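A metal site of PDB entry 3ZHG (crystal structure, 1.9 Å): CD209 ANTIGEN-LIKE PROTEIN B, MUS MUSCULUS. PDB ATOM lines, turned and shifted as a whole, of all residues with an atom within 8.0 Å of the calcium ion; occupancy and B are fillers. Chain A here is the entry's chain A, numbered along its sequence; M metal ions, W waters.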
ATOM      1  N   TRP A  98      -2.549 -19.170  21.192  1.00  0.00           N
ATOM      2  CA  TRP A  98      -3.759 -18.860  20.415  1.00  0.00           C
ATOM      3  C   TRP A  98      -3.770 -19.534  19.052  1.00  0.00           C
ATOM      4  O   TRP A  98      -2.882 -19.308  18.235  1.00  0.00           O
ATOM      5  CB  TRP A  98      -3.903 -17.338  20.281  1.00  0.00           C
ATOM      6  CG  TRP A  98      -3.970 -16.697  21.629  1.00  0.00           C
ATOM      7  CD1 TRP A  98      -2.918 -16.207  22.361  1.00  0.00           C
ATOM      8  CD2 TRP A  98      -5.127 -16.535  22.450  1.00  0.00           C
ATOM      9  NE1 TRP A  98      -3.362 -15.731  23.573  1.00  0.00           N
ATOM     10  CE2 TRP A  98      -4.715 -15.929  23.642  1.00  0.00           C
ATOM     11  CE3 TRP A  98      -6.488 -16.838  22.262  1.00  0.00           C
ATOM     12  CZ2 TRP A  98      -5.616 -15.611  24.655  1.00  0.00           C
ATOM     13  CZ3 TRP A  98      -7.367 -16.531  23.277  1.00  0.00           C
ATOM     14  CH2 TRP A  98      -6.930 -15.932  24.459  1.00  0.00           C
ATOM     15  N   TRP A 114      -4.118  -7.177  18.683  1.00  0.00           N
ATOM     16  CA  TRP A 114      -4.601  -7.141  20.062  1.00  0.00           C
ATOM     17  C   TRP A 114      -4.725  -5.701  20.553  1.00  0.00           C
ATOM     18  O   TRP A 114      -3.827  -4.890  20.326  1.00  0.00           O
ATOM     19  CB  TRP A 114      -3.633  -7.849  21.001  1.00  0.00           C
ATOM     20  CG  TRP A 114      -3.570  -9.346  20.902  1.00  0.00           C
ATOM     21  CD1 TRP A 114      -2.508 -10.091  20.473  1.00  0.00           C
ATOM     22  CD2 TRP A 114      -4.590 -10.282  21.282  1.00  0.00           C
ATOM     23  NE1 TRP A 114      -2.811 -11.429  20.547  1.00  0.00           N
ATOM     24  CE2 TRP A 114      -4.086 -11.569  21.037  1.00  0.00           C
ATOM     25  CE3 TRP A 114      -5.884 -10.155  21.793  1.00  0.00           C
ATOM     26  CZ2 TRP A 114      -4.823 -12.720  21.290  1.00  0.00           C
ATOM     27  CZ3 TRP A 114      -6.610 -11.299  22.051  1.00  0.00           C
ATOM     28  CH2 TRP A 114      -6.083 -12.571  21.793  1.00  0.00           C
ATOM     29  N   GLY A 117      -3.455  -3.984  26.460  1.00  0.00           N
ATOM     30  CA  GLY A 117      -3.952  -4.682  27.630  1.00  0.00           C
ATOM     31  C   GLY A 117      -4.523  -6.059  27.344  1.00  0.00           C
ATOM     32  O   GLY A 117      -4.976  -6.749  28.249  1.00  0.00           O
ATOM     33  N   GLU A 118      -4.494  -6.474  26.077  1.00  0.00           N
ATOM     34  CA  GLU A 118      -4.975  -7.797  25.686  1.00  0.00           C
ATOM     35  C   GLU A 118      -3.853  -8.572  25.024  1.00  0.00           C
ATOM     36  O   GLU A 118      -2.975  -7.987  24.398  1.00  0.00           O
ATOM     37  CB  GLU A 118      -6.151  -7.666  24.711  1.00  0.00           C
ATOM     38  CG  GLU A 118      -7.304  -6.824  25.233  1.00  0.00           C
ATOM     39  CD  GLU A 118      -8.193  -7.572  26.211  1.00  0.00           C
ATOM     40  OE1 GLU A 118      -8.333  -8.815  26.097  1.00  0.00           O
ATOM     41  OE2 GLU A 118      -8.784  -6.913  27.095  1.00  0.00           O
ATOM     42  N   PRO A 119      -3.880  -9.903  25.149  1.00  0.00           N
ATOM     43  CA  PRO A 119      -4.882 -10.668  25.882  1.00  0.00           C
ATOM     44  C   PRO A 119      -4.632 -10.662  27.377  1.00  0.00           C
ATOM     45  O   PRO A 119      -3.471 -10.645  27.791  1.00  0.00           O
ATOM     46  CB  PRO A 119      -4.701 -12.080  25.338  1.00  0.00           C
ATOM     47  CG  PRO A 119      -3.275 -12.129  24.943  1.00  0.00           C
ATOM     48  CD  PRO A 119      -2.978 -10.775  24.380  1.00  0.00           C
ATOM     49  N   ASN A 120      -5.691 -10.697  28.185  1.00  0.00           N
ATOM     50  CA  ASN A 120      -5.504 -10.784  29.646  1.00  0.00           C
ATOM     51  C   ASN A 120      -6.417 -11.833  30.250  1.00  0.00           C
ATOM     52  O   ASN A 120      -6.988 -12.657  29.532  1.00  0.00           O
ATOM     53  CB  ASN A 120      -5.748  -9.422  30.303  1.00  0.00           C
ATOM     54  CG  ASN A 120      -7.160  -8.950  30.136  1.00  0.00           C
ATOM     55  OD1 ASN A 120      -7.954  -9.595  29.446  1.00  0.00           O
ATOM     56  ND2 ASN A 120      -7.495  -7.826  30.752  1.00  0.00           N
ATOM     57  N   ASN A 121      -6.571 -11.804  31.570  1.00  0.00           N
ATOM     58  CA  ASN A 121      -7.439 -12.773  32.230  1.00  0.00           C
ATOM     59  C   ASN A 121      -7.200 -14.159  31.655  1.00  0.00           C
ATOM     60  O   ASN A 121      -8.133 -14.865  31.282  1.00  0.00           O
ATOM     61  CB  ASN A 121      -8.896 -12.375  32.061  1.00  0.00           C
ATOM     62  CG  ASN A 121      -9.221 -11.080  32.778  1.00  0.00           C
ATOM     63  OD1 ASN A 121      -8.918 -10.938  33.961  1.00  0.00           O
ATOM     64  ND2 ASN A 121      -9.851 -10.139  32.081  1.00  0.00           N
ATOM     65  N   ILE A 122      -5.928 -14.549  31.596  1.00  0.00           N
ATOM     66  CA  ILE A 122      -5.525 -15.749  30.872  1.00  0.00           C
ATOM     67  C   ILE A 122      -6.058 -17.001  31.559  1.00  0.00           C
ATOM     68  O   ILE A 122      -5.929 -17.153  32.768  1.00  0.00           O
ATOM     69  CB  ILE A 122      -3.998 -15.849  30.739  1.00  0.00           C
ATOM     70  CG1 ILE A 122      -3.468 -14.696  29.881  1.00  0.00           C
ATOM     71  CG2 ILE A 122      -3.589 -17.176  30.134  1.00  0.00           C
ATOM     72  CD1 ILE A 122      -3.772 -14.830  28.398  1.00  0.00           C
ATOM     73  N   GLU A 124      -9.191 -17.628  31.772  1.00  0.00           N
ATOM     74  CA  GLU A 124     -10.583 -17.328  32.100  1.00  0.00           C
ATOM     75  C   GLU A 124     -11.341 -16.802  30.873  1.00  0.00           C
ATOM     76  O   GLU A 124     -12.526 -17.094  30.681  1.00  0.00           O
ATOM     77  CB  GLU A 124     -10.683 -16.335  33.263  1.00  0.00           C
ATOM     78  CG  GLU A 124     -12.014 -15.582  33.313  1.00  0.00           C
ATOM     79  CD  GLU A 124     -12.083 -14.543  34.443  1.00  0.00           C
ATOM     80  OE1 GLU A 124     -11.124 -13.739  34.601  1.00  0.00           O
ATOM     81  OE2 GLU A 124     -13.100 -14.532  35.170  1.00  0.00           O
ATOM     82  N   GLU A 125     -10.634 -16.018  30.060  1.00  0.00           N
ATOM     83  CA  GLU A 125     -11.192 -15.487  28.819  1.00  0.00           C
ATOM     84  C   GLU A 125     -10.470 -16.142  27.653  1.00  0.00           C
ATOM     85  O   GLU A 125      -9.354 -15.761  27.307  1.00  0.00           O
ATOM     86  CB  GLU A 125     -11.038 -13.962  28.793  1.00  0.00           C
ATOM     87  CG  GLU A 125     -11.796 -13.279  29.927  1.00  0.00           C
ATOM     88  CD  GLU A 125     -11.845 -11.759  29.794  1.00  0.00           C
ATOM     89  OE1 GLU A 125     -10.865 -11.161  29.298  1.00  0.00           O
ATOM     90  OE2 GLU A 125     -12.865 -11.162  30.194  1.00  0.00           O
ATOM     91  N   ASP A 126     -11.104 -17.147  27.058  1.00  0.00           N
ATOM     92  CA  ASP A 126     -10.418 -18.051  26.149  1.00  0.00           C
ATOM     93  C   ASP A 126     -10.739 -17.878  24.669  1.00  0.00           C
ATOM     94  O   ASP A 126     -10.132 -18.532  23.821  1.00  0.00           O
ATOM     95  CB  ASP A 126     -10.701 -19.507  26.544  1.00  0.00           C
ATOM     96  CG  ASP A 126     -10.064 -19.870  27.866  1.00  0.00           C
ATOM     97  OD1 ASP A 126      -8.843 -19.636  28.030  1.00  0.00           O
ATOM     98  OD2 ASP A 126     -10.776 -20.395  28.740  1.00  0.00           O
ATOM     99  N   CYS A 127     -11.683 -17.014  24.337  1.00  0.00           N
ATOM    100  CA  CYS A 127     -12.051 -16.820  22.941  1.00  0.00           C
ATOM    101  C   CYS A 127     -11.850 -15.366  22.539  1.00  0.00           C
ATOM    102  O   CYS A 127     -11.955 -14.480  23.377  1.00  0.00           O
ATOM    103  CB  CYS A 127     -13.501 -17.243  22.712  1.00  0.00           C
ATOM    104  SG  CYS A 127     -13.820 -18.979  23.113  1.00  0.00           S
ATOM    105  N   GLU A 129     -12.540 -11.813  20.285  1.00  0.00           N
ATOM    106  CA  GLU A 129     -13.559 -10.992  19.628  1.00  0.00           C
ATOM    107  C   GLU A 129     -12.959  -9.742  19.011  1.00  0.00           C
ATOM    108  O   GLU A 129     -11.935  -9.228  19.485  1.00  0.00           O
ATOM    109  CB  GLU A 129     -14.578 -10.549  20.674  1.00  0.00           C
ATOM    110  CG  GLU A 129     -13.958  -9.638  21.723  1.00  0.00           C
ATOM    111  CD  GLU A 129     -14.952  -9.004  22.661  1.00  0.00           C
ATOM    112  OE1 GLU A 129     -16.158  -9.347  22.608  1.00  0.00           O
ATOM    113  OE2 GLU A 129     -14.541  -8.170  23.484  1.00  0.00           O
ATOM    114  N   TRP A 135      -8.541  -6.497  19.039  1.00  0.00           N
ATOM    115  CA  TRP A 135      -9.008  -7.772  19.555  1.00  0.00           C
ATOM    116  C   TRP A 135      -8.919  -7.819  21.076  1.00  0.00           C
ATOM    117  O   TRP A 135      -7.922  -7.379  21.652  1.00  0.00           O
ATOM    118  CB  TRP A 135      -8.180  -8.925  19.009  1.00  0.00           C
ATOM    119  CG  TRP A 135      -8.027  -8.994  17.519  1.00  0.00           C
ATOM    120  CD1 TRP A 135      -8.643  -8.206  16.596  1.00  0.00           C
ATOM    121  CD2 TRP A 135      -7.190  -9.908  16.775  1.00  0.00           C
ATOM    122  NE1 TRP A 135      -8.250  -8.577  15.323  1.00  0.00           N
ATOM    123  CE2 TRP A 135      -7.358  -9.623  15.418  1.00  0.00           C
ATOM    124  CE3 TRP A 135      -6.331 -10.946  17.151  1.00  0.00           C
ATOM    125  CZ2 TRP A 135      -6.697 -10.332  14.411  1.00  0.00           C
ATOM    126  CZ3 TRP A 135      -5.666 -11.654  16.153  1.00  0.00           C
ATOM    127  CH2 TRP A 135      -5.855 -11.334  14.800  1.00  0.00           C
ATOM    128  N   ASN A 136      -9.948  -8.378  21.699  1.00  0.00           N
ATOM    129  CA  ASN A 136      -9.914  -8.704  23.123  1.00  0.00           C
ATOM    130  C   ASN A 136     -10.041 -10.198  23.232  1.00  0.00           C
ATOM    131  O   ASN A 136     -10.593 -10.827  22.329  1.00  0.00           O
ATOM    132  CB  ASN A 136     -11.139  -8.126  23.842  1.00  0.00           C
ATOM    133  CG  ASN A 136     -11.061  -6.634  24.022  1.00  0.00           C
ATOM    134  OD1 ASN A 136     -10.122  -5.984  23.559  1.00  0.00           O
ATOM    135  ND2 ASN A 136     -12.038  -6.069  24.719  1.00  0.00           N
ATOM    136  N   ASP A 137      -9.564 -10.796  24.321  1.00  0.00           N
ATOM    137  CA  ASP A 137     -10.056 -12.135  24.648  1.00  0.00           C
ATOM    138  C   ASP A 137     -11.263 -11.955  25.566  1.00  0.00           C
ATOM    139  O   ASP A 137     -11.344 -10.975  26.322  1.00  0.00           O
ATOM    140  CB  ASP A 137      -8.963 -13.035  25.250  1.00  0.00           C
ATOM    141  CG  ASP A 137      -8.401 -12.504  26.552  1.00  0.00           C
ATOM    142  OD1 ASP A 137      -8.763 -11.383  26.948  1.00  0.00           O
ATOM    143  OD2 ASP A 137      -7.596 -13.227  27.180  1.00  0.00           O
ATOM    144  N   SER A 138     -12.229 -12.863  25.462  1.00  0.00           N
ATOM    145  CA  SER A 138     -13.458 -12.760  26.225  1.00  0.00           C
ATOM    146  C   SER A 138     -13.911 -14.129  26.706  1.00  0.00           C
ATOM    147  O   SER A 138     -13.425 -15.156  26.239  1.00  0.00           O
ATOM    148  CB  SER A 138     -14.591 -12.150  25.376  1.00  0.00           C
ATOM    149  OG  SER A 138     -14.150 -10.979  24.711  1.00  0.00           O
ATOM    150  N   LYS A 139     -14.860 -14.146  27.638  1.00  0.00           N
ATOM    151  CA  LYS A 139     -15.458 -15.400  28.089  1.00  0.00           C
ATOM    152  C   LYS A 139     -16.263 -16.048  26.949  1.00  0.00           C
ATOM    153  O   LYS A 139     -17.218 -15.462  26.433  1.00  0.00           O
ATOM    154  CB  LYS A 139     -16.361 -15.149  29.279  1.00  0.00           C
ATOM    155  CG  LYS A 139     -15.614 -14.787  30.569  1.00  0.00           C
ATOM    156  CD  LYS A 139     -16.584 -14.233  31.620  1.00  0.00           C
ATOM    157  CE  LYS A 139     -16.669 -15.135  32.835  1.00  0.00           C
ATOM    158  NZ  LYS A 139     -15.418 -15.063  33.665  1.00  0.00           N
HETATM  159 CA    CA M   1      -9.900  -9.552  27.936  1.00  0.00          CA
HETATM  160  O   HOH W   1     -11.395  -7.939  27.601  1.00  0.00           O
HETATM  161  O   HOH W   2     -10.674  -7.642  29.856  1.00  0.00           O
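The side-chain carboxylate of Glu 125 sits close to the side-chain amide nitrogen of Asn 121 (3.1 Å). The side-chain amide oxygen (OD1) of Asn 120 lies close to the side-chain amide nitrogen (ND2) of Asn 121 (3.3 Å).
The calcium ion is bound by water W1, at 2.2 Å. OE1 of Glu 125 binds the calcium ion (2.3 Å). The side-chain carboxylate (OD1) of Asp 137 is bound to the calcium ion. OD1 of Asn 120 binds the calcium ion. OE1 of Glu 118 binds the calcium ion (2.5 Å). O of Asp 137 binds the calcium ion, 2.6 Å away. The calcium ion is bound by water W2 (2.8 Å). The calcium ion has seven donor atoms within binding distance. Slightly farther from the calcium ion lies OE2 of Glu 118 (3.0 Å).
Water W2 lies within hydrogen-bond range of the side-chain amide nitrogen of Asn 120, the side-chain carboxylate of Glu 118 and the side-chain amide nitrogen of Asn 121. Water W1 bridges the side-chain carboxylate of Glu 118 (2.9 Å) and the side-chain amide nitrogen of Asn 136 (3.5 Å).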
